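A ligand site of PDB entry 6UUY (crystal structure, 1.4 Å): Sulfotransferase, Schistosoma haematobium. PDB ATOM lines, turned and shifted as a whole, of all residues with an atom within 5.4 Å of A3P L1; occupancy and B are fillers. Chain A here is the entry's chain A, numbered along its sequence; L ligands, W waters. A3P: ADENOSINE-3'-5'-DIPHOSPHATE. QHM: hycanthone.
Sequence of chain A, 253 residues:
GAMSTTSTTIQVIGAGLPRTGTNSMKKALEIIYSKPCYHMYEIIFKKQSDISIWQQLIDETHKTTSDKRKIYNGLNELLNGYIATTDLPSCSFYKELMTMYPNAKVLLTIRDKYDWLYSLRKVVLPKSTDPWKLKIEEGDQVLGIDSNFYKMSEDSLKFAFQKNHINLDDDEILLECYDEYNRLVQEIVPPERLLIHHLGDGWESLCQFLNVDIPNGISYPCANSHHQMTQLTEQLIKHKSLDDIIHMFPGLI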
ATOM      1  N   LEU A  17      33.874   5.395 -26.971  1.00  0.00           N
ATOM      2  CA  LEU A  17      33.669   6.553 -27.835  1.00  0.00           C
ATOM      3  C   LEU A  17      32.173   6.806 -28.046  1.00  0.00           C
ATOM      4  O   LEU A  17      31.339   5.918 -27.836  1.00  0.00           O
ATOM      5  CB  LEU A  17      34.349   6.293 -29.182  1.00  0.00           C
ATOM      6  CG  LEU A  17      35.868   6.263 -29.103  1.00  0.00           C
ATOM      7  CD1 LEU A  17      36.451   5.657 -30.392  1.00  0.00           C
ATOM      8  CD2 LEU A  17      36.415   7.663 -28.878  1.00  0.00           C
ATOM      9  N   PRO A  18      31.804   8.007 -28.497  1.00  0.00           N
ATOM     10  CA  PRO A  18      30.394   8.260 -28.828  1.00  0.00           C
ATOM     11  C   PRO A  18      29.851   7.282 -29.860  1.00  0.00           C
ATOM     12  O   PRO A  18      30.569   6.799 -30.740  1.00  0.00           O
ATOM     13  CB  PRO A  18      30.382   9.709 -29.336  1.00  0.00           C
ATOM     14  CG  PRO A  18      31.780  10.091 -29.529  1.00  0.00           C
ATOM     15  CD  PRO A  18      32.623   9.230 -28.649  1.00  0.00           C
ATOM     16  N   ARG A  19      28.556   6.999 -29.735  1.00  0.00           N
ATOM     17  CA  ARG A  19      27.812   6.068 -30.572  1.00  0.00           C
ATOM     18  C   ARG A  19      28.144   4.611 -30.270  1.00  0.00           C
ATOM     19  O   ARG A  19      27.891   3.737 -31.105  1.00  0.00           O
ATOM     20  CB  ARG A  19      27.862   6.389 -32.078  1.00  0.00           C
ATOM     21  CG  ARG A  19      27.584   7.854 -32.441  1.00  0.00           C
ATOM     22  CD  ARG A  19      26.310   8.401 -31.774  1.00  0.00           C
ATOM     23  NE  ARG A  19      25.119   7.739 -32.271  1.00  0.00           N
ATOM     24  CZ  ARG A  19      23.893   7.905 -31.765  1.00  0.00           C
ATOM     25  NH1 ARG A  19      23.698   8.710 -30.724  1.00  0.00           N
ATOM     26  NH2 ARG A  19      22.864   7.266 -32.299  1.00  0.00           N
ATOM     27  N   THR A  20      28.691   4.308 -29.087  1.00  0.00           N
ATOM     28  CA  THR A  20      28.922   2.941 -28.641  1.00  0.00           C
ATOM     29  C   THR A  20      27.998   2.561 -27.481  1.00  0.00           C
ATOM     30  O   THR A  20      28.286   1.599 -26.769  1.00  0.00           O
ATOM     31  CB  THR A  20      30.378   2.711 -28.251  1.00  0.00           C
ATOM     32  OG1 THR A  20      30.715   3.522 -27.117  1.00  0.00           O
ATOM     33  CG2 THR A  20      31.339   3.015 -29.409  1.00  0.00           C
ATOM     34  N   GLY A  21      26.906   3.292 -27.265  1.00  0.00           N
ATOM     35  CA  GLY A  21      26.048   3.021 -26.140  1.00  0.00           C
ATOM     36  C   GLY A  21      26.389   3.791 -24.880  1.00  0.00           C
ATOM     37  O   GLY A  21      26.043   3.341 -23.778  1.00  0.00           O
ATOM     38  N   THR A  22      27.036   4.963 -25.024  1.00  0.00           N
ATOM     39  CA  THR A  22      27.472   5.706 -23.838  1.00  0.00           C
ATOM     40  C   THR A  22      26.289   6.282 -23.066  1.00  0.00           C
ATOM     41  O   THR A  22      26.325   6.372 -21.837  1.00  0.00           O
ATOM     42  CB  THR A  22      28.438   6.830 -24.203  1.00  0.00           C
ATOM     43  OG1 THR A  22      27.792   7.808 -25.028  1.00  0.00           O
ATOM     44  CG2 THR A  22      29.670   6.285 -24.912  1.00  0.00           C
ATOM     45  N   ASN A  23      25.230   6.707 -23.773  1.00  0.00           N
ATOM     46  CA  ASN A  23      24.104   7.266 -23.040  1.00  0.00           C
ATOM     47  C   ASN A  23      23.372   6.190 -22.248  1.00  0.00           C
ATOM     48  O   ASN A  23      22.936   6.426 -21.108  1.00  0.00           O
ATOM     49  CB  ASN A  23      23.151   8.014 -23.961  1.00  0.00           C
ATOM     50  CG  ASN A  23      22.190   8.858 -23.193  1.00  0.00           C
ATOM     51  OD1 ASN A  23      21.047   8.470 -23.009  1.00  0.00           O
ATOM     52  ND2 ASN A  23      22.644  10.017 -22.742  1.00  0.00           N
ATOM     53  N   SER A  24      23.213   5.011 -22.837  1.00  0.00           N
ATOM     54  CA  SER A  24      22.622   3.897 -22.088  1.00  0.00           C
ATOM     55  C   SER A  24      23.478   3.527 -20.887  1.00  0.00           C
ATOM     56  O   SER A  24      22.949   3.236 -19.806  1.00  0.00           O
ATOM     57  CB  SER A  24      22.430   2.683 -22.987  1.00  0.00           C
ATOM     58  OG  SER A  24      21.385   2.900 -23.913  1.00  0.00           O
ATOM     59  N   HIS A  39      28.292  12.899 -19.182  1.00  0.00           N
ATOM     60  CA  HIS A  39      28.046  12.561 -20.575  1.00  0.00           C
ATOM     61  C   HIS A  39      28.036  13.870 -21.356  1.00  0.00           C
ATOM     62  O   HIS A  39      27.859  14.943 -20.774  1.00  0.00           O
ATOM     63  CB  HIS A  39      26.680  11.853 -20.736  1.00  0.00           C
ATOM     64  CG  HIS A  39      26.452  11.249 -22.090  1.00  0.00           C
ATOM     65  ND1 HIS A  39      25.831  11.945 -23.113  1.00  0.00           N
ATOM     66  CD2 HIS A  39      26.748  10.024 -22.586  1.00  0.00           C
ATOM     67  CE1 HIS A  39      25.769  11.167 -24.183  1.00  0.00           C
ATOM     68  NE2 HIS A  39      26.314   9.991 -23.882  1.00  0.00           N
ATOM     69  N   ARG A 111      31.382  -1.632 -30.146  1.00  0.00           N
ATOM     70  CA  ARG A 111      30.454  -2.226 -31.098  1.00  0.00           C
ATOM     71  C   ARG A 111      31.175  -2.428 -32.427  1.00  0.00           C
ATOM     72  O   ARG A 111      32.306  -1.965 -32.631  1.00  0.00           O
ATOM     73  CB  ARG A 111      29.215  -1.350 -31.289  1.00  0.00           C
ATOM     74  CG  ARG A 111      29.502  -0.133 -32.135  1.00  0.00           C
ATOM     75  CD  ARG A 111      28.333   0.838 -32.170  1.00  0.00           C
ATOM     76  NE  ARG A 111      27.160   0.308 -32.853  1.00  0.00           N
ATOM     77  CZ  ARG A 111      26.062   1.007 -33.095  1.00  0.00           C
ATOM     78  NH1 ARG A 111      26.016   2.299 -32.753  1.00  0.00           N
ATOM     79  NH2 ARG A 111      25.005   0.455 -33.688  1.00  0.00           N
ATOM     80  N   ASP A 115      28.924  -0.511 -38.045  1.00  0.00           N
ATOM     81  CA  ASP A 115      27.732   0.025 -37.400  1.00  0.00           C
ATOM     82  C   ASP A 115      28.040   1.356 -36.738  1.00  0.00           C
ATOM     83  O   ASP A 115      27.248   2.311 -36.820  1.00  0.00           O
ATOM     84  CB  ASP A 115      27.218  -0.942 -36.340  1.00  0.00           C
ATOM     85  CG  ASP A 115      26.656  -2.233 -36.892  1.00  0.00           C
ATOM     86  OD1 ASP A 115      26.316  -2.305 -38.095  1.00  0.00           O
ATOM     87  OD2 ASP A 115      26.508  -3.186 -36.096  1.00  0.00           O
ATOM     88  N   SER A 119      26.450   5.218 -37.584  1.00  0.00           N
ATOM     89  CA  SER A 119      25.818   5.959 -36.504  1.00  0.00           C
ATOM     90  C   SER A 119      26.487   7.317 -36.296  1.00  0.00           C
ATOM     91  O   SER A 119      25.817   8.349 -36.155  1.00  0.00           O
ATOM     92  CB  SER A 119      25.880   5.112 -35.232  1.00  0.00           C
ATOM     93  OG  SER A 119      25.154   5.710 -34.169  1.00  0.00           O
ATOM     94  N   VAL A 123      24.650  11.194 -36.940  1.00  0.00           N
ATOM     95  CA  VAL A 123      24.239  11.877 -35.712  1.00  0.00           C
ATOM     96  C   VAL A 123      25.221  12.979 -35.302  1.00  0.00           C
ATOM     97  O   VAL A 123      24.812  14.097 -35.000  1.00  0.00           O
ATOM     98  CB  VAL A 123      24.009  10.885 -34.553  1.00  0.00           C
ATOM     99  CG1 VAL A 123      23.568  11.641 -33.303  1.00  0.00           C
ATOM    100  CG2 VAL A 123      22.994   9.834 -34.942  1.00  0.00           C
ATOM    101  N   LEU A 199      27.804  -3.876 -27.220  1.00  0.00           N
ATOM    102  CA  LEU A 199      26.415  -3.465 -27.382  1.00  0.00           C
ATOM    103  C   LEU A 199      25.508  -4.682 -27.265  1.00  0.00           C
ATOM    104  O   LEU A 199      25.714  -5.673 -27.964  1.00  0.00           O
ATOM    105  CB  LEU A 199      26.258  -2.792 -28.753  1.00  0.00           C
ATOM    106  CG  LEU A 199      25.298  -1.608 -28.841  1.00  0.00           C
ATOM    107  CD1 LEU A 199      25.523  -0.568 -27.737  1.00  0.00           C
ATOM    108  CD2 LEU A 199      25.403  -0.959 -30.212  1.00  0.00           C
ATOM    109  N   GLY A 200      24.554  -4.611 -26.340  1.00  0.00           N
ATOM    110  CA  GLY A 200      23.656  -5.718 -26.068  1.00  0.00           C
ATOM    111  C   GLY A 200      24.011  -6.579 -24.871  1.00  0.00           C
ATOM    112  O   GLY A 200      23.223  -7.464 -24.516  1.00  0.00           O
ATOM    113  N   TYR A 220      17.976  -3.085 -18.757  1.00  0.00           N
ATOM    114  CA  TYR A 220      19.127  -2.296 -19.155  1.00  0.00           C
ATOM    115  C   TYR A 220      18.687  -1.235 -20.177  1.00  0.00           C
ATOM    116  O   TYR A 220      17.958  -1.561 -21.115  1.00  0.00           O
ATOM    117  CB  TYR A 220      20.203  -3.203 -19.748  1.00  0.00           C
ATOM    118  CG  TYR A 220      21.470  -2.448 -20.006  1.00  0.00           C
ATOM    119  CD1 TYR A 220      22.429  -2.314 -19.017  1.00  0.00           C
ATOM    120  CD2 TYR A 220      21.693  -1.825 -21.234  1.00  0.00           C
ATOM    121  CE1 TYR A 220      23.585  -1.592 -19.237  1.00  0.00           C
ATOM    122  CE2 TYR A 220      22.832  -1.091 -21.461  1.00  0.00           C
ATOM    123  CZ  TYR A 220      23.785  -0.985 -20.461  1.00  0.00           C
ATOM    124  OH  TYR A 220      24.912  -0.262 -20.704  1.00  0.00           O
ATOM    125  N   PRO A 221      19.121   0.023 -20.027  1.00  0.00           N
ATOM    126  CA  PRO A 221      18.619   1.090 -20.914  1.00  0.00           C
ATOM    127  C   PRO A 221      18.975   0.869 -22.379  1.00  0.00           C
ATOM    128  O   PRO A 221      20.011   0.288 -22.729  1.00  0.00           O
ATOM    129  CB  PRO A 221      19.306   2.347 -20.376  1.00  0.00           C
ATOM    130  CG  PRO A 221      19.610   2.025 -18.948  1.00  0.00           C
ATOM    131  CD  PRO A 221      19.940   0.555 -18.932  1.00  0.00           C
ATOM    132  N   CYS A 222      18.108   1.367 -23.253  1.00  0.00           N
ATOM    133  CA  CYS A 222      18.323   1.303 -24.698  1.00  0.00           C
ATOM    134  C   CYS A 222      18.003   2.676 -25.296  1.00  0.00           C
ATOM    135  O   CYS A 222      16.993   2.889 -25.957  1.00  0.00           O
ATOM    136  CB  CYS A 222      17.479   0.199 -25.340  1.00  0.00           C
ATOM    137  SG  CYS A 222      17.948  -0.148 -27.030  1.00  0.00           S
ATOM    138  N   ALA A 223      18.885   3.633 -25.062  1.00  0.00           N
ATOM    139  CA  ALA A 223      18.635   5.033 -25.366  1.00  0.00           C
ATOM    140  C   ALA A 223      19.468   5.513 -26.556  1.00  0.00           C
ATOM    141  O   ALA A 223      20.499   4.941 -26.895  1.00  0.00           O
ATOM    142  CB  ALA A 223      19.000   5.884 -24.146  1.00  0.00           C
ATOM    143  N   ASN A 224      18.987   6.593 -27.198  1.00  0.00           N
ATOM    144  CA  ASN A 224      19.821   7.435 -28.058  1.00  0.00           C
ATOM    145  C   ASN A 224      20.088   6.825 -29.433  1.00  0.00           C
ATOM    146  O   ASN A 224      21.180   6.977 -29.987  1.00  0.00           O
ATOM    147  CB  ASN A 224      21.144   7.771 -27.329  1.00  0.00           C
ATOM    148  CG  ASN A 224      21.740   9.119 -27.736  1.00  0.00           C
ATOM    149  OD1 ASN A 224      21.035  10.001 -28.200  1.00  0.00           O
ATOM    150  ND2 ASN A 224      23.043   9.280 -27.526  1.00  0.00           N
ATOM    151  N   SER A 225      19.088   6.159 -30.011  1.00  0.00           N
ATOM    152  CA  SER A 225      19.238   5.557 -31.326  1.00  0.00           C
ATOM    153  C   SER A 225      19.348   6.623 -32.414  1.00  0.00           C
ATOM    154  O   SER A 225      18.898   7.764 -32.269  1.00  0.00           O
ATOM    155  CB  SER A 225      18.039   4.662 -31.636  1.00  0.00           C
ATOM    156  OG  SER A 225      16.881   5.446 -31.929  1.00  0.00           O
ATOM    157  N   HIS A 226      19.949   6.235 -33.558  1.00  0.00           N
ATOM    158  CA  HIS A 226      20.045   7.182 -34.658  1.00  0.00           C
ATOM    159  C   HIS A 226      18.681   7.557 -35.202  1.00  0.00           C
ATOM    160  O   HIS A 226      18.491   8.684 -35.678  1.00  0.00           O
ATOM    161  CB  HIS A 226      21.000   6.705 -35.774  1.00  0.00           C
ATOM    162  CG  HIS A 226      20.488   5.567 -36.605  1.00  0.00           C
ATOM    163  ND1 HIS A 226      19.512   5.726 -37.568  1.00  0.00           N
ATOM    164  CD2 HIS A 226      20.827   4.266 -36.621  1.00  0.00           C
ATOM    165  CE1 HIS A 226      19.275   4.562 -38.146  1.00  0.00           C
ATOM    166  NE2 HIS A 226      20.064   3.656 -37.586  1.00  0.00           N
ATOM    167  N   HIS A 227      17.712   6.643 -35.137  1.00  0.00           N
ATOM    168  CA  HIS A 227      16.360   6.974 -35.578  1.00  0.00           C
ATOM    169  C   HIS A 227      15.797   8.121 -34.749  1.00  0.00           C
ATOM    170  O   HIS A 227      15.253   9.093 -35.287  1.00  0.00           O
ATOM    171  CB  HIS A 227      15.463   5.743 -35.464  1.00  0.00           C
ATOM    172  CG  HIS A 227      15.715   4.714 -36.533  1.00  0.00           C
ATOM    173  ND1 HIS A 227      16.257   3.473 -36.266  1.00  0.00           N
ATOM    174  CD2 HIS A 227      15.495   4.752 -37.866  1.00  0.00           C
ATOM    175  CE1 HIS A 227      16.356   2.786 -37.393  1.00  0.00           C
ATOM    176  NE2 HIS A 227      15.897   3.535 -38.371  1.00  0.00           N
HETATM  177  P1  A3P L   1      22.431   3.431 -33.456  1.00  0.00           P
HETATM  178  O1P A3P L   1      22.974   2.378 -34.385  1.00  0.00           O
HETATM  179  O2P A3P L   1      20.949   3.290 -33.172  1.00  0.00           O
HETATM  180  O3P A3P L   1      22.760   4.847 -33.823  1.00  0.00           O
HETATM  181  P2  A3P L   1      25.685   6.784 -27.747  1.00  0.00           P
HETATM  182  O4P A3P L   1      27.111   6.531 -27.311  1.00  0.00           O
HETATM  183  O5P A3P L   1      25.572   7.905 -28.735  1.00  0.00           O
HETATM  184  O6P A3P L   1      24.677   6.904 -26.613  1.00  0.00           O
HETATM  185  O5' A3P L   1      25.292   5.437 -28.522  1.00  0.00           O
HETATM  186  C5' A3P L   1      24.033   5.270 -29.191  1.00  0.00           C
HETATM  187  C4' A3P L   1      24.024   3.978 -29.991  1.00  0.00           C
HETATM  188  O4' A3P L   1      23.994   2.854 -29.093  1.00  0.00           O
HETATM  189  C3' A3P L   1      22.795   3.898 -30.860  1.00  0.00           C
HETATM  190  O3' A3P L   1      23.136   3.155 -32.029  1.00  0.00           O
HETATM  191  C2' A3P L   1      21.876   3.059 -29.981  1.00  0.00           C
HETATM  192  O2' A3P L   1      20.814   2.426 -30.693  1.00  0.00           O
HETATM  193  C1' A3P L   1      22.863   2.057 -29.418  1.00  0.00           C
HETATM  194  N9  A3P L   1      22.399   1.437 -28.162  1.00  0.00           N
HETATM  195  C8  A3P L   1      22.296   2.057 -26.969  1.00  0.00           C
HETATM  196  N7  A3P L   1      21.858   1.193 -26.013  1.00  0.00           N
HETATM  197  C5  A3P L   1      21.664   0.004 -26.600  1.00  0.00           C
HETATM  198  C6  A3P L   1      21.219  -1.332 -26.175  1.00  0.00           C
HETATM  199  N6  A3P L   1      20.852  -1.562 -24.898  1.00  0.00           N
HETATM  200  N1  A3P L   1      21.158  -2.295 -27.115  1.00  0.00           N
HETATM  201  C2  A3P L   1      21.522  -2.074 -28.396  1.00  0.00           C
HETATM  202  N3  A3P L   1      21.942  -0.885 -28.862  1.00  0.00           N
HETATM  203  C4  A3P L   1      22.027   0.171 -28.012  1.00  0.00           C
HETATM  204  N1  QHM L   2      26.375  17.263 -31.189  1.00  0.00           N
HETATM  205  C4  QHM L   2      28.101  14.026 -28.979  1.00  0.00           C
HETATM  206  C5  QHM L   2      32.574  14.882 -31.758  1.00  0.00           C
HETATM  207  C6  QHM L   2      33.185  15.627 -32.741  1.00  0.00           C
HETATM  208  C7  QHM L   2      32.514  16.644 -33.385  1.00  0.00           C
HETATM  209  C8  QHM L   2      31.205  16.932 -33.030  1.00  0.00           C
HETATM  210  C10 QHM L   2      28.313  15.797 -30.661  1.00  0.00           C
HETATM  211  C13 QHM L   2      30.565  16.193 -32.036  1.00  0.00           C
HETATM  212  C15 QHM L   2      24.927  17.558 -31.021  1.00  0.00           C
HETATM  213  C17 QHM L   2      22.238  17.218 -30.401  1.00  0.00           C
HETATM  214  C20 QHM L   2      20.406  16.337 -32.560  1.00  0.00           C
HETATM  215  C9  QHM L   2      29.112  16.572 -31.696  1.00  0.00           C
HETATM  216  C3  QHM L   2      26.810  14.416 -28.774  1.00  0.00           C
HETATM  217  C2  QHM L   2      26.231  15.441 -29.463  1.00  0.00           C
HETATM  218  C12 QHM L   2      31.254  15.161 -31.401  1.00  0.00           C
HETATM  219  C11 QHM L   2      28.834  14.720 -29.914  1.00  0.00           C
HETATM  220  C1  QHM L   2      26.962  16.146 -30.418  1.00  0.00           C
HETATM  221  N2  QHM L   2      22.668  16.903 -31.761  1.00  0.00           N
HETATM  222  C14 QHM L   2      28.714  12.865 -28.188  1.00  0.00           C
HETATM  223  O1  QHM L   2      28.529  17.645 -32.359  1.00  0.00           O
HETATM  224  C16 QHM L   2      24.103  16.528 -31.807  1.00  0.00           C
HETATM  225  C18 QHM L   2      22.128  15.971 -29.501  1.00  0.00           C
HETATM  226  C19 QHM L   2      21.848  15.857 -32.374  1.00  0.00           C
HETATM  227  O2  QHM L   2      27.725  12.198 -27.430  1.00  0.00           O
HETATM  228  S1  QHM L   2      30.528  14.141 -30.102  1.00  0.00           S
HETATM  229  O   HOH W   1      19.840  -4.699 -26.755  1.00  0.00           O
HETATM  230  O   HOH W   2      21.706  -0.042 -34.542  1.00  0.00           O
HETATM  231  O   HOH W   3      25.562  10.678 -28.237  1.00  0.00           O
HETATM  232  O   HOH W   4      20.471  -4.398 -23.692  1.00  0.00           O
HETATM  233  O   HOH W   5      23.138   4.903 -25.704  1.00  0.00           O
HETATM  234  O   HOH W   6      24.397   2.094 -36.791  1.00  0.00           O
HETATM  235  O   HOH W   7      21.777  -1.333 -31.760  1.00  0.00           O
HETATM  236  O   HOH W   8      19.040   1.677 -34.103  1.00  0.00           O
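OG of Ser 119 lies within hydrogen-bond range of O3P of A3P L1 (2.6 Å). The backbone NH (N) of Thr 22 is in hydrogen-bond range of an oxygen (O4P) of A3P L1 (2.8 Å). OG1 of Thr 22 sits at hydrogen-bond distance from O4P of A3P L1. A nitrogen (N7) of A3P L1 lies within hydrogen-bond range of the side-chain hydroxyl (OG) of Ser 24 (2.7 Å). An oxygen (O4P) of A3P L1 is in hydrogen-bond range of the backbone NH of Arg 19 (2.9 Å). NH1 of Arg 19 lies within salt-bridge range of O5P of A3P L1 (2.8 Å). The guanidinium group of Arg 111 lies within salt-bridge range of an oxygen (O1P) of A3P L1 (2.9 Å). N of Asn 23 lies within hydrogen-bond range of O6P of A3P L1 (2.9 Å). The backbone NH (N) of Gly 21 lies within hydrogen-bond range of an oxygen (O5') of A3P L1 (3.0 Å). The backbone carbonyl oxygen of Pro 221 is in hydrogen-bond range of a nitrogen (N6) of A3P L1, at 3.0 Å. ND2 of Asn 224 sits at hydrogen-bond distance from O6P of A3P L1, at 3.0 Å. O2P of A3P L1 is in hydrogen-bond range of N of His 226, at 3.1 Å. The backbone NH (N) of Thr 20 lies within hydrogen-bond range of an oxygen (O4P) of A3P L1, 3.3 Å away.
Water W5 lies within hydrogen-bond range of O6P of A3P L1 (2.7 Å), N of Ser 24 (2.9 Å), O of Ala 223 (2.9 Å) and N of Asn 23 (3.4 Å). Water W2 lies within hydrogen-bond range of an oxygen (O1P) of A3P L1 (2.7 Å) and the guanidinium group (NH2) of Arg 111 (3.4 Å). Water W6 lies within hydrogen-bond range of an oxygen (O1P) of A3P L1 (2.8 Å) and the backbone carbonyl oxygen (O) of Asp 115 (2.9 Å). Water W3 lies within hydrogen-bond range of O2 of QHM L2 (2.8 Å), O5P of A3P L1 (2.8 Å) and ND2 of Asn 224 (3.0 Å).
Pro 18 touches A3P L1 (C to O4P, 3.8 Å). Leu 199 touches A3P L1 (CG to N3, 3.4 Å). Tyr 220 touches A3P L1 (CD2 to N6, 3.8 Å). SG of Cys 222 touches C6 of A3P L1, 3.6 Å away. O of Ala 223 touches C8 of A3P L1, 3.4 Å away. CA of Ser 225 touches O2P of A3P L1, 3.4 Å away. 17 residues have an atom within 4 Å of A3P L1: Pro 18, Arg 19, Thr 20, Gly 21, Thr 22, Asn 23, Ser 24, Arg 111, Ser 119, Leu 199, Tyr 220, Pro 221, Cys 222, Ala 223, Asn 224, Ser 225 and His 226.
The guanidinium group of Arg 19 is in hydrogen-bond range of the side-chain hydroxyl of Ser 119 (2.8 Å). OG1 of Thr 22 sits at hydrogen-bond distance from NE2 of His 39 (2.9 Å). OG of Ser 24 is in hydrogen-bond range of O of Pro 221, 3.2 Å away. The backbone NH of Ala 223 lies within hydrogen-bond range of the side-chain hydroxyl of Ser 24, at 2.8 Å. The guanidinium group (NH1) of Arg 111 sits at hydrogen-bond distance from the backbone carbonyl oxygen (O) of Arg 19. The guanidinium group of Arg 19 lies within hydrogen-bond range of the backbone carbonyl oxygen of Asn 224 (2.9 Å). The backbone NH (N) of Asn 23 is in hydrogen-bond range of a ring nitrogen (NE2) of His 39 (3.5 Å). The side-chain hydroxyl (OG1) of Thr 20 lies within hydrogen-bond range of the backbone carbonyl oxygen (O) of Leu 17, 2.6 Å away.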
